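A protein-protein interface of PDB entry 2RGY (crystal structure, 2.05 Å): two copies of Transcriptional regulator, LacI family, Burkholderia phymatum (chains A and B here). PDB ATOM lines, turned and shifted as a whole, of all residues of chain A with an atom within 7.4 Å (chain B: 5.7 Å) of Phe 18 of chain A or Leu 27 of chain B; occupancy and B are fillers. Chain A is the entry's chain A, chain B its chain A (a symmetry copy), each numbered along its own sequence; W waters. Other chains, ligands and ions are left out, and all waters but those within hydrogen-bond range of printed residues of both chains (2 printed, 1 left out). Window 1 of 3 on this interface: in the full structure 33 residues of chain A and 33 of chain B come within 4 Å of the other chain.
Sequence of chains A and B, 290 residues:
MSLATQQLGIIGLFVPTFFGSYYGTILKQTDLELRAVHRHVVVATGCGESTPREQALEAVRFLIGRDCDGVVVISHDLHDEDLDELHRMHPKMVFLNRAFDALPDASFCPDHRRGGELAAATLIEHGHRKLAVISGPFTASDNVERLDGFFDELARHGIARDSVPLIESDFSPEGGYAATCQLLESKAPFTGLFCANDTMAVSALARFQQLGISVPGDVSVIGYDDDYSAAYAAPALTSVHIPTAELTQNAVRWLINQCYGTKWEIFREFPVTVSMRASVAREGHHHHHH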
ATOM      1  N   LEU A  13       6.056 -27.450  28.306  1.00  0.00           N
ATOM      2  CA  LEU A  13       7.503 -27.613  28.361  1.00  0.00           C
ATOM      3  C   LEU A  13       8.244 -26.526  27.590  1.00  0.00           C
ATOM      4  O   LEU A  13       8.006 -26.331  26.400  1.00  0.00           O
ATOM      5  CB  LEU A  13       7.910 -28.973  27.788  1.00  0.00           C
ATOM      6  CG  LEU A  13       9.404 -29.152  27.480  1.00  0.00           C
ATOM      7  CD1 LEU A  13      10.232 -29.025  28.752  1.00  0.00           C
ATOM      8  CD2 LEU A  13       9.626 -30.517  26.842  1.00  0.00           C
ATOM      9  N   VAL A  15      11.909 -25.118  26.251  1.00  0.00           N
ATOM     10  CA  VAL A  15      13.301 -25.431  25.975  1.00  0.00           C
ATOM     11  C   VAL A  15      13.777 -24.248  25.134  1.00  0.00           C
ATOM     12  O   VAL A  15      13.038 -23.740  24.282  1.00  0.00           O
ATOM     13  CB  VAL A  15      13.464 -26.745  25.180  1.00  0.00           C
ATOM     14  CG1 VAL A  15      13.046 -27.925  26.034  1.00  0.00           C
ATOM     15  CG2 VAL A  15      12.641 -26.689  23.904  1.00  0.00           C
ATOM     16  N   PRO A  16      15.005 -23.779  25.374  1.00  0.00           N
ATOM     17  CA  PRO A  16      15.530 -22.641  24.613  1.00  0.00           C
ATOM     18  C   PRO A  16      15.711 -22.884  23.118  1.00  0.00           C
ATOM     19  O   PRO A  16      15.896 -21.930  22.359  1.00  0.00           O
ATOM     20  CB  PRO A  16      16.842 -22.331  25.321  1.00  0.00           C
ATOM     21  CG  PRO A  16      17.265 -23.672  25.850  1.00  0.00           C
ATOM     22  CD  PRO A  16      15.981 -24.248  26.371  1.00  0.00           C
ATOM     23  N   THR A  17      15.647 -24.146  22.695  1.00  0.00           N
ATOM     24  CA  THR A  17      15.809 -24.499  21.282  1.00  0.00           C
ATOM     25  C   THR A  17      15.539 -25.992  21.077  1.00  0.00           C
ATOM     26  O   THR A  17      15.693 -26.779  22.006  1.00  0.00           O
ATOM     27  CB  THR A  17      17.246 -24.165  20.795  1.00  0.00           C
ATOM     28  OG1 THR A  17      17.353 -24.388  19.382  1.00  0.00           O
ATOM     29  CG2 THR A  17      18.271 -25.027  21.522  1.00  0.00           C
ATOM     30  N   PHE A  18      15.110 -26.371  19.876  1.00  0.00           N
ATOM     31  CA  PHE A  18      14.829 -27.774  19.566  1.00  0.00           C
ATOM     32  C   PHE A  18      16.077 -28.498  19.083  1.00  0.00           C
ATOM     33  O   PHE A  18      16.054 -29.712  18.891  1.00  0.00           O
ATOM     34  CB  PHE A  18      13.767 -27.885  18.470  1.00  0.00           C
ATOM     35  CG  PHE A  18      12.399 -27.453  18.896  1.00  0.00           C
ATOM     36  CD1 PHE A  18      11.635 -28.256  19.742  1.00  0.00           C
ATOM     37  CD2 PHE A  18      11.860 -26.251  18.430  1.00  0.00           C
ATOM     38  CE1 PHE A  18      10.339 -27.873  20.126  1.00  0.00           C
ATOM     39  CE2 PHE A  18      10.566 -25.846  18.800  1.00  0.00           C
ATOM     40  CZ  PHE A  18       9.798 -26.662  19.653  1.00  0.00           C
ATOM     41  N   PHE A  19      17.160 -27.755  18.872  1.00  0.00           N
ATOM     42  CA  PHE A  19      18.399 -28.348  18.379  1.00  0.00           C
ATOM     43  C   PHE A  19      19.400 -28.775  19.437  1.00  0.00           C
ATOM     44  O   PHE A  19      19.527 -28.144  20.481  1.00  0.00           O
ATOM     45  CB  PHE A  19      19.074 -27.388  17.410  1.00  0.00           C
ATOM     46  CG  PHE A  19      18.190 -26.974  16.272  1.00  0.00           C
ATOM     47  CD1 PHE A  19      17.527 -25.746  16.295  1.00  0.00           C
ATOM     48  CD2 PHE A  19      18.000 -27.829  15.189  1.00  0.00           C
ATOM     49  CE1 PHE A  19      16.676 -25.369  15.246  1.00  0.00           C
ATOM     50  CE2 PHE A  19      17.154 -27.473  14.130  1.00  0.00           C
ATOM     51  CZ  PHE A  19      16.490 -26.240  14.157  1.00  0.00           C
ATOM     52  N   GLY A  20      20.137 -29.841  19.125  1.00  0.00           N
ATOM     53  CA  GLY A  20      21.118 -30.388  20.044  1.00  0.00           C
ATOM     54  C   GLY A  20      20.489 -31.622  20.657  1.00  0.00           C
ATOM     55  O   GLY A  20      19.334 -31.564  21.075  1.00  0.00           O
ATOM     56  N   SER A  21      21.208 -32.741  20.702  1.00  0.00           N
ATOM     57  CA  SER A  21      20.641 -33.956  21.278  1.00  0.00           C
ATOM     58  C   SER A  21      20.343 -33.809  22.775  1.00  0.00           C
ATOM     59  O   SER A  21      19.603 -34.599  23.360  1.00  0.00           O
ATOM     60  CB  SER A  21      21.576 -35.145  21.034  1.00  0.00           C
ATOM     61  OG  SER A  21      22.862 -34.913  21.581  1.00  0.00           O
ATOM     62  N   TYR A  22      20.925 -32.784  23.390  1.00  0.00           N
ATOM     63  CA  TYR A  22      20.709 -32.512  24.809  1.00  0.00           C
ATOM     64  C   TYR A  22      19.240 -32.118  24.991  1.00  0.00           C
ATOM     65  O   TYR A  22      18.535 -32.666  25.835  1.00  0.00           O
ATOM     66  CB  TYR A  22      21.620 -31.369  25.270  1.00  0.00           C
ATOM     67  CG  TYR A  22      21.396 -30.949  26.700  1.00  0.00           C
ATOM     68  CD1 TYR A  22      21.850 -31.734  27.765  1.00  0.00           C
ATOM     69  CD2 TYR A  22      20.718 -29.769  26.989  1.00  0.00           C
ATOM     70  CE1 TYR A  22      21.630 -31.341  29.092  1.00  0.00           C
ATOM     71  CE2 TYR A  22      20.496 -29.370  28.300  1.00  0.00           C
ATOM     72  CZ  TYR A  22      20.952 -30.159  29.348  1.00  0.00           C
ATOM     73  OH  TYR A  22      20.705 -29.749  30.639  1.00  0.00           O
ATOM     74  N   TYR A  23      18.773 -31.167  24.187  1.00  0.00           N
ATOM     75  CA  TYR A  23      17.387 -30.748  24.295  1.00  0.00           C
ATOM     76  C   TYR A  23      16.462 -31.822  23.743  1.00  0.00           C
ATOM     77  O   TYR A  23      15.335 -31.960  24.204  1.00  0.00           O
ATOM     78  CB  TYR A  23      17.179 -29.411  23.589  1.00  0.00           C
ATOM     79  CG  TYR A  23      17.910 -28.299  24.303  1.00  0.00           C
ATOM     80  CD1 TYR A  23      17.534 -27.912  25.587  1.00  0.00           C
ATOM     81  CD2 TYR A  23      19.024 -27.693  23.732  1.00  0.00           C
ATOM     82  CE1 TYR A  23      18.256 -26.950  26.293  1.00  0.00           C
ATOM     83  CE2 TYR A  23      19.756 -26.729  24.425  1.00  0.00           C
ATOM     84  CZ  TYR A  23      19.364 -26.364  25.708  1.00  0.00           C
ATOM     85  OH  TYR A  23      20.088 -25.422  26.411  1.00  0.00           O
ATOM     86  N   GLY A  24      16.940 -32.588  22.766  1.00  0.00           N
ATOM     87  CA  GLY A  24      16.126 -33.658  22.221  1.00  0.00           C
ATOM     88  C   GLY A  24      15.842 -34.686  23.304  1.00  0.00           C
ATOM     89  O   GLY A  24      14.750 -35.251  23.374  1.00  0.00           O
ATOM     90  N   LEU A  27      13.127 -33.397  25.570  1.00  0.00           N
ATOM     91  CA  LEU A  27      11.839 -33.478  24.890  1.00  0.00           C
ATOM     92  C   LEU A  27      11.348 -34.921  24.875  1.00  0.00           C
ATOM     93  O   LEU A  27      10.183 -35.199  25.169  1.00  0.00           O
ATOM     94  CB  LEU A  27      11.954 -32.984  23.443  1.00  0.00           C
ATOM     95  CG  LEU A  27      12.511 -31.576  23.209  1.00  0.00           C
ATOM     96  CD1 LEU A  27      12.654 -31.342  21.723  1.00  0.00           C
ATOM     97  CD2 LEU A  27      11.592 -30.537  23.835  1.00  0.00           C
ATOM     98  N   VAL A  43       4.912 -27.986  23.630  1.00  0.00           N
ATOM     99  CA  VAL A  43       6.260 -27.446  23.693  1.00  0.00           C
ATOM    100  C   VAL A  43       6.303 -26.009  23.210  1.00  0.00           C
ATOM    101  O   VAL A  43       5.533 -25.602  22.332  1.00  0.00           O
ATOM    102  CB  VAL A  43       7.254 -28.271  22.841  1.00  0.00           C
ATOM    103  CG1 VAL A  43       8.676 -27.727  23.020  1.00  0.00           C
ATOM    104  CG2 VAL A  43       7.198 -29.729  23.248  1.00  0.00           C
ATOM    105  N   ALA A  44       7.212 -25.244  23.800  1.00  0.00           N
ATOM    106  CA  ALA A  44       7.390 -23.855  23.435  1.00  0.00           C
ATOM    107  C   ALA A  44       8.877 -23.523  23.526  1.00  0.00           C
ATOM    108  O   ALA A  44       9.573 -24.016  24.413  1.00  0.00           O
ATOM    109  CB  ALA A  44       6.596 -22.971  24.370  1.00  0.00           C
ATOM    110  N   THR A  45       9.363 -22.717  22.591  1.00  0.00           N
ATOM    111  CA  THR A  45      10.757 -22.304  22.591  1.00  0.00           C
ATOM    112  C   THR A  45      10.804 -20.800  22.363  1.00  0.00           C
ATOM    113  O   THR A  45       9.772 -20.174  22.119  1.00  0.00           O
ATOM    114  CB  THR A  45      11.565 -23.016  21.494  1.00  0.00           C
ATOM    115  OG1 THR A  45      12.951 -22.679  21.647  1.00  0.00           O
ATOM    116  CG2 THR A  45      11.089 -22.593  20.101  1.00  0.00           C
ATOM    117  N   GLY A  46      11.993 -20.214  22.454  1.00  0.00           N
ATOM    118  CA  GLY A  46      12.108 -18.779  22.262  1.00  0.00           C
ATOM    119  C   GLY A  46      11.836 -18.307  20.843  1.00  0.00           C
ATOM    120  O   GLY A  46      12.469 -18.787  19.900  1.00  0.00           O
ATOM    121  N   CYS A  47      10.909 -17.352  20.706  1.00  0.00           N
ATOM    122  CA  CYS A  47      10.513 -16.768  19.418  1.00  0.00           C
ATOM    123  C   CYS A  47      10.518 -15.231  19.458  1.00  0.00           C
ATOM    124  O   CYS A  47      10.389 -14.622  20.525  1.00  0.00           O
ATOM    125  CB  CYS A  47       9.084 -17.198  19.034  1.00  0.00           C
ATOM    126  SG  CYS A  47       8.793 -18.963  18.833  1.00  0.00           S
ATOM    127  N   LEU B  13       1.323 -32.429  16.291  1.00  0.00           N
ATOM    128  CA  LEU B  13       2.444 -32.672  15.392  1.00  0.00           C
ATOM    129  C   LEU B  13       3.155 -33.988  15.685  1.00  0.00           C
ATOM    130  O   LEU B  13       3.609 -34.217  16.805  1.00  0.00           O
ATOM    131  CB  LEU B  13       3.467 -31.537  15.495  1.00  0.00           C
ATOM    132  CG  LEU B  13       4.839 -31.811  14.861  1.00  0.00           C
ATOM    133  CD1 LEU B  13       4.699 -32.046  13.363  1.00  0.00           C
ATOM    134  CD2 LEU B  13       5.759 -30.625  15.125  1.00  0.00           C
ATOM    135  N   VAL B  15       6.346 -36.478  14.773  1.00  0.00           N
ATOM    136  CA  VAL B  15       7.658 -36.591  14.160  1.00  0.00           C
ATOM    137  C   VAL B  15       8.181 -37.931  14.672  1.00  0.00           C
ATOM    138  O   VAL B  15       7.968 -38.290  15.838  1.00  0.00           O
ATOM    139  CB  VAL B  15       8.610 -35.454  14.588  1.00  0.00           C
ATOM    140  CG1 VAL B  15       8.123 -34.131  14.032  1.00  0.00           C
ATOM    141  CG2 VAL B  15       8.705 -35.394  16.104  1.00  0.00           C
ATOM    142  N   THR B  17      10.998 -38.774  15.571  1.00  0.00           N
ATOM    143  CA  THR B  17      12.041 -38.610  16.590  1.00  0.00           C
ATOM    144  C   THR B  17      12.369 -37.127  16.775  1.00  0.00           C
ATOM    145  O   THR B  17      12.167 -36.332  15.862  1.00  0.00           O
ATOM    146  CB  THR B  17      13.330 -39.375  16.181  1.00  0.00           C
ATOM    147  OG1 THR B  17      14.294 -39.321  17.242  1.00  0.00           O
ATOM    148  CG2 THR B  17      13.933 -38.769  14.919  1.00  0.00           C
ATOM    149  N   PHE B  18      12.843 -36.754  17.961  1.00  0.00           N
ATOM    150  CA  PHE B  18      13.198 -35.364  18.247  1.00  0.00           C
ATOM    151  C   PHE B  18      14.636 -35.063  17.847  1.00  0.00           C
ATOM    152  O   PHE B  18      15.067 -33.914  17.905  1.00  0.00           O
ATOM    153  CB  PHE B  18      13.052 -35.062  19.740  1.00  0.00           C
ATOM    154  CG  PHE B  18      11.637 -35.055  20.228  1.00  0.00           C
ATOM    155  CD1 PHE B  18      10.785 -33.997  19.912  1.00  0.00           C
ATOM    156  CD2 PHE B  18      11.160 -36.096  21.028  1.00  0.00           C
ATOM    157  CE1 PHE B  18       9.464 -33.967  20.389  1.00  0.00           C
ATOM    158  CE2 PHE B  18       9.842 -36.089  21.516  1.00  0.00           C
ATOM    159  CZ  PHE B  18       8.987 -35.017  21.197  1.00  0.00           C
ATOM    160  N   TYR B  22      17.042 -31.921  11.157  1.00  0.00           N
ATOM    161  CA  TYR B  22      15.978 -31.992  10.158  1.00  0.00           C
ATOM    162  C   TYR B  22      14.638 -31.943  10.899  1.00  0.00           C
ATOM    163  O   TYR B  22      13.762 -31.146  10.575  1.00  0.00           O
ATOM    164  CB  TYR B  22      16.089 -33.296   9.362  1.00  0.00           C
ATOM    165  CG  TYR B  22      14.971 -33.505   8.373  1.00  0.00           C
ATOM    166  CD1 TYR B  22      14.919 -32.782   7.174  1.00  0.00           C
ATOM    167  CD2 TYR B  22      13.956 -34.417   8.640  1.00  0.00           C
ATOM    168  CE1 TYR B  22      13.873 -32.976   6.265  1.00  0.00           C
ATOM    169  CE2 TYR B  22      12.914 -34.617   7.744  1.00  0.00           C
ATOM    170  CZ  TYR B  22      12.875 -33.893   6.559  1.00  0.00           C
ATOM    171  OH  TYR B  22      11.823 -34.098   5.694  1.00  0.00           O
ATOM    172  N   TYR B  23      14.482 -32.795  11.908  1.00  0.00           N
ATOM    173  CA  TYR B  23      13.241 -32.800  12.663  1.00  0.00           C
ATOM    174  C   TYR B  23      13.153 -31.566  13.548  1.00  0.00           C
ATOM    175  O   TYR B  23      12.061 -31.078  13.816  1.00  0.00           O
ATOM    176  CB  TYR B  23      13.119 -34.084  13.478  1.00  0.00           C
ATOM    177  CG  TYR B  23      12.955 -35.286  12.577  1.00  0.00           C
ATOM    178  CD1 TYR B  23      11.815 -35.434  11.792  1.00  0.00           C
ATOM    179  CD2 TYR B  23      13.970 -36.228  12.448  1.00  0.00           C
ATOM    180  CE1 TYR B  23      11.690 -36.490  10.889  1.00  0.00           C
ATOM    181  CE2 TYR B  23      13.860 -37.290  11.551  1.00  0.00           C
ATOM    182  CZ  TYR B  23      12.714 -37.412  10.774  1.00  0.00           C
ATOM    183  OH  TYR B  23      12.598 -38.450   9.871  1.00  0.00           O
ATOM    184  N   GLY B  24      14.299 -31.057  13.991  1.00  0.00           N
ATOM    185  CA  GLY B  24      14.290 -29.857  14.807  1.00  0.00           C
ATOM    186  C   GLY B  24      13.731 -28.695  14.001  1.00  0.00           C
ATOM    187  O   GLY B  24      13.011 -27.844  14.526  1.00  0.00           O
ATOM    188  N   THR B  25      14.063 -28.660  12.715  1.00  0.00           N
ATOM    189  CA  THR B  25      13.590 -27.603  11.821  1.00  0.00           C
ATOM    190  C   THR B  25      12.070 -27.637  11.696  1.00  0.00           C
ATOM    191  O   THR B  25      11.403 -26.605  11.709  1.00  0.00           O
ATOM    192  CB  THR B  25      14.197 -27.770  10.412  1.00  0.00           C
ATOM    193  OG1 THR B  25      15.627 -27.736  10.516  1.00  0.00           O
ATOM    194  CG2 THR B  25      13.723 -26.655   9.484  1.00  0.00           C
ATOM    195  N   ILE B  26      11.535 -28.845  11.568  1.00  0.00           N
ATOM    196  CA  ILE B  26      10.100 -29.037  11.437  1.00  0.00           C
ATOM    197  C   ILE B  26       9.405 -28.600  12.716  1.00  0.00           C
ATOM    198  O   ILE B  26       8.375 -27.932  12.663  1.00  0.00           O
ATOM    199  CB  ILE B  26       9.794 -30.512  11.142  1.00  0.00           C
ATOM    200  CG1 ILE B  26      10.420 -30.895   9.802  1.00  0.00           C
ATOM    201  CG2 ILE B  26       8.299 -30.757  11.112  1.00  0.00           C
ATOM    202  CD1 ILE B  26      10.360 -32.368   9.509  1.00  0.00           C
ATOM    203  N   LEU B  27       9.979 -28.964  13.859  1.00  0.00           N
ATOM    204  CA  LEU B  27       9.409 -28.590  15.150  1.00  0.00           C
ATOM    205  C   LEU B  27       9.445 -27.075  15.314  1.00  0.00           C
ATOM    206  O   LEU B  27       8.459 -26.458  15.727  1.00  0.00           O
ATOM    207  CB  LEU B  27      10.200 -29.227  16.299  1.00  0.00           C
ATOM    208  CG  LEU B  27      10.370 -30.749  16.295  1.00  0.00           C
ATOM    209  CD1 LEU B  27      11.276 -31.149  17.436  1.00  0.00           C
ATOM    210  CD2 LEU B  27       9.014 -31.429  16.416  1.00  0.00           C
ATOM    211  N   LYS B  28      10.587 -26.475  14.998  1.00  0.00           N
ATOM    212  CA  LYS B  28      10.734 -25.034  15.142  1.00  0.00           C
ATOM    213  C   LYS B  28       9.731 -24.259  14.294  1.00  0.00           C
ATOM    214  O   LYS B  28       9.036 -23.391  14.812  1.00  0.00           O
ATOM    215  CB  LYS B  28      12.163 -24.607  14.788  1.00  0.00           C
ATOM    216  CG  LYS B  28      12.426 -23.101  14.885  1.00  0.00           C
ATOM    217  CD  LYS B  28      13.876 -22.784  14.483  1.00  0.00           C
ATOM    218  CE  LYS B  28      14.132 -21.277  14.349  1.00  0.00           C
ATOM    219  NZ  LYS B  28      15.509 -20.977  13.803  1.00  0.00           N
ATOM    220  N   GLN B  29       9.657 -24.569  13.002  1.00  0.00           N
ATOM    221  CA  GLN B  29       8.728 -23.882  12.103  1.00  0.00           C
ATOM    222  C   GLN B  29       7.269 -24.074  12.493  1.00  0.00           C
ATOM    223  O   GLN B  29       6.471 -23.157  12.353  1.00  0.00           O
ATOM    224  CB  GLN B  29       8.902 -24.350  10.660  1.00  0.00           C
ATOM    225  CG  GLN B  29      10.118 -23.794   9.963  1.00  0.00           C
ATOM    226  CD  GLN B  29      10.210 -22.285  10.072  1.00  0.00           C
ATOM    227  OE1 GLN B  29       9.259 -21.564   9.782  1.00  0.00           O
ATOM    228  NE2 GLN B  29      11.362 -21.806  10.499  1.00  0.00           N
ATOM    229  N   THR B  30       6.912 -25.267  12.961  1.00  0.00           N
ATOM    230  CA  THR B  30       5.532 -25.515  13.356  1.00  0.00           C
ATOM    231  C   THR B  30       5.220 -24.636  14.570  1.00  0.00           C
ATOM    232  O   THR B  30       4.210 -23.939  14.595  1.00  0.00           O
ATOM    233  CB  THR B  30       5.303 -27.005  13.716  1.00  0.00           C
ATOM    234  OG1 THR B  30       5.698 -27.835  12.618  1.00  0.00           O
ATOM    235  CG2 THR B  30       3.829 -27.258  14.017  1.00  0.00           C
ATOM    236  N   ASP B  31       6.101 -24.662  15.567  1.00  0.00           N
ATOM    237  CA  ASP B  31       5.930 -23.861  16.782  1.00  0.00           C
ATOM    238  C   ASP B  31       5.802 -22.381  16.422  1.00  0.00           C
ATOM    239  O   ASP B  31       4.942 -21.672  16.942  1.00  0.00           O
ATOM    240  CB  ASP B  31       7.131 -24.078  17.721  1.00  0.00           C
ATOM    241  CG  ASP B  31       7.100 -23.173  18.957  1.00  0.00           C
ATOM    242  OD1 ASP B  31       6.025 -23.031  19.578  1.00  0.00           O
ATOM    243  OD2 ASP B  31       8.162 -22.614  19.323  1.00  0.00           O
ATOM    244  N   LEU B  32       6.657 -21.946  15.505  1.00  0.00           N
ATOM    245  CA  LEU B  32       6.715 -20.568  15.031  1.00  0.00           C
ATOM    246  C   LEU B  32       5.414 -20.075  14.397  1.00  0.00           C
ATOM    247  O   LEU B  32       4.875 -19.037  14.790  1.00  0.00           O
ATOM    248  CB  LEU B  32       7.862 -20.449  14.024  1.00  0.00           C
ATOM    249  CG  LEU B  32       8.770 -19.223  14.031  1.00  0.00           C
ATOM    250  CD1 LEU B  32       9.137 -18.865  15.460  1.00  0.00           C
ATOM    251  CD2 LEU B  32      10.040 -19.518  13.213  1.00  0.00           C
ATOM    252  N   VAL B  43       3.309 -32.026  20.690  1.00  0.00           N
ATOM    253  CA  VAL B  43       4.153 -32.912  19.907  1.00  0.00           C
ATOM    254  C   VAL B  43       4.066 -34.342  20.404  1.00  0.00           C
ATOM    255  O   VAL B  43       3.873 -34.597  21.599  1.00  0.00           O
ATOM    256  CB  VAL B  43       5.638 -32.478  19.945  1.00  0.00           C
ATOM    257  CG1 VAL B  43       6.471 -33.378  19.025  1.00  0.00           C
ATOM    258  CG2 VAL B  43       5.765 -31.031  19.514  1.00  0.00           C
HETATM  259  O   HOH W   1       9.922 -21.880  17.083  1.00  0.00           O
HETATM  260  O   HOH W   2      16.684 -31.356  16.445  1.00  0.00           O
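Water W1 lies within hydrogen-bond range of the backbone carbonyl oxygen of Lys 28 of chain B, the side-chain carboxylate of Asp 31 of chain B and the side-chain sulfur of Cys 47 of chain A. Water W2 lies within hydrogen-bond range of the backbone carbonyl oxygen (O) of Phe 18 of chain A (3.0 Å), the backbone carbonyl oxygen (O) of Phe 18 of chain B (3.4 Å) and the backbone NH (N) of Gly 24 of chain B (3.4 Å).
The backbone carbonyl oxygen (O) of Val 15 of chain A lies within hydrogen-bond range of the side-chain hydroxyl (OG1) of Thr 45 of chain A, at 2.8 Å. The side-chain hydroxyl (OG1) of Thr 45 of chain A is in hydrogen-bond range of the backbone carbonyl oxygen (O) of Pro 16 of chain A, 3.1 Å away. OG1 of Thr 17 of chain A sits close to N of Phe 19 of chain A, 3.4 Å away. N of Thr 17 of chain A lies within hydrogen-bond range of OG1 of Thr 45 of chain A (3.2 Å). O of Thr 45 of chain A is in hydrogen-bond range of SG of Cys 47 of chain A.
Hydrophobic or aromatic side chains of chain A within 4 Å of the printed part of chain B: Phe 18, Phe 19 and Leu 27. Of the 16 printed residues of chain B, 7 touch a printed residue of chain A. Printed residues of chain B that touch a printed residue of chain A: Phe 18, Gly 24, Thr 25, Leu 27, Lys 28, Asp 31 and Leu 32. Hydrophobic or aromatic side chains of chain B that line the printed part of chain A: Phe 18, Leu 27 and Leu 32. Among the printed residues, 10 pairs touch across the chains. Among the printed residues, no Asp or Glu carboxylate lies within 4 Å of a Lys or Arg side-chain nitrogen of the other chain.
Printed residues of chain B within 4 Å of Phe 18 of chain A: Leu 27 (3.7 Å) and Lys 28 (3.7 Å). Of the printed residues of chain A, Leu 32 of chain B touches Cys 47. Of the printed residues of chain A, Thr 25 of chain B touches Phe 19. Printed residues of chain B within 4 Å of Cys 47 of chain A: Asp 31 (3.7 Å) and Leu 32 (3.4 Å). Printed residues of chain A within 4 Å of Phe 18 of chain B: Leu 27. Printed residues of chain B within 4 Å of Leu 27 of chain A: Phe 18 (3.7 Å). Val 15 of chain A touches none of the printed residues of chain B. The nearest printed residue of chain B that does not touch Val 43 of chain A is Val 43 of chain B (4.2 Å).
Phe 18 of chain A touches Leu 27 of chain B, and with the chains exchanged Leu 27 of chain A touches Phe 18 of chain B. Positions printed for both chains: 13, 15, 17, 18, 22, 23, 24, 27 and 43.
Among the printed residues, pairs that only touch across the chains: Phe 18 of chain A with Leu 27 of chain B (3.7 Å), Phe 18 of chain A with Lys 28 of chain B (3.7 Å), Phe 19 of chain A with Gly 24 of chain B (3.6 Å), Phe 19 of chain A with Thr 25 of chain B (3.6 Å), Phe 19 of chain A with Lys 28 of chain B (3.9 Å), Leu 27 of chain A with Phe 18 of chain B (3.7 Å), Val 43 of chain A with Asp 31 of chain B (3.8 Å) and Cys 47 of chain A with Leu 32 of chain B (3.4 Å).
N of Thr 45 of chain A sits close to OD2 of Asp 31 of chain B (3.5 Å). The side-chain sulfur (SG) of Cys 47 of chain A is in hydrogen-bond range of the side-chain carboxylate (OD2) of Asp 31 of chain B, 3.7 Å away.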
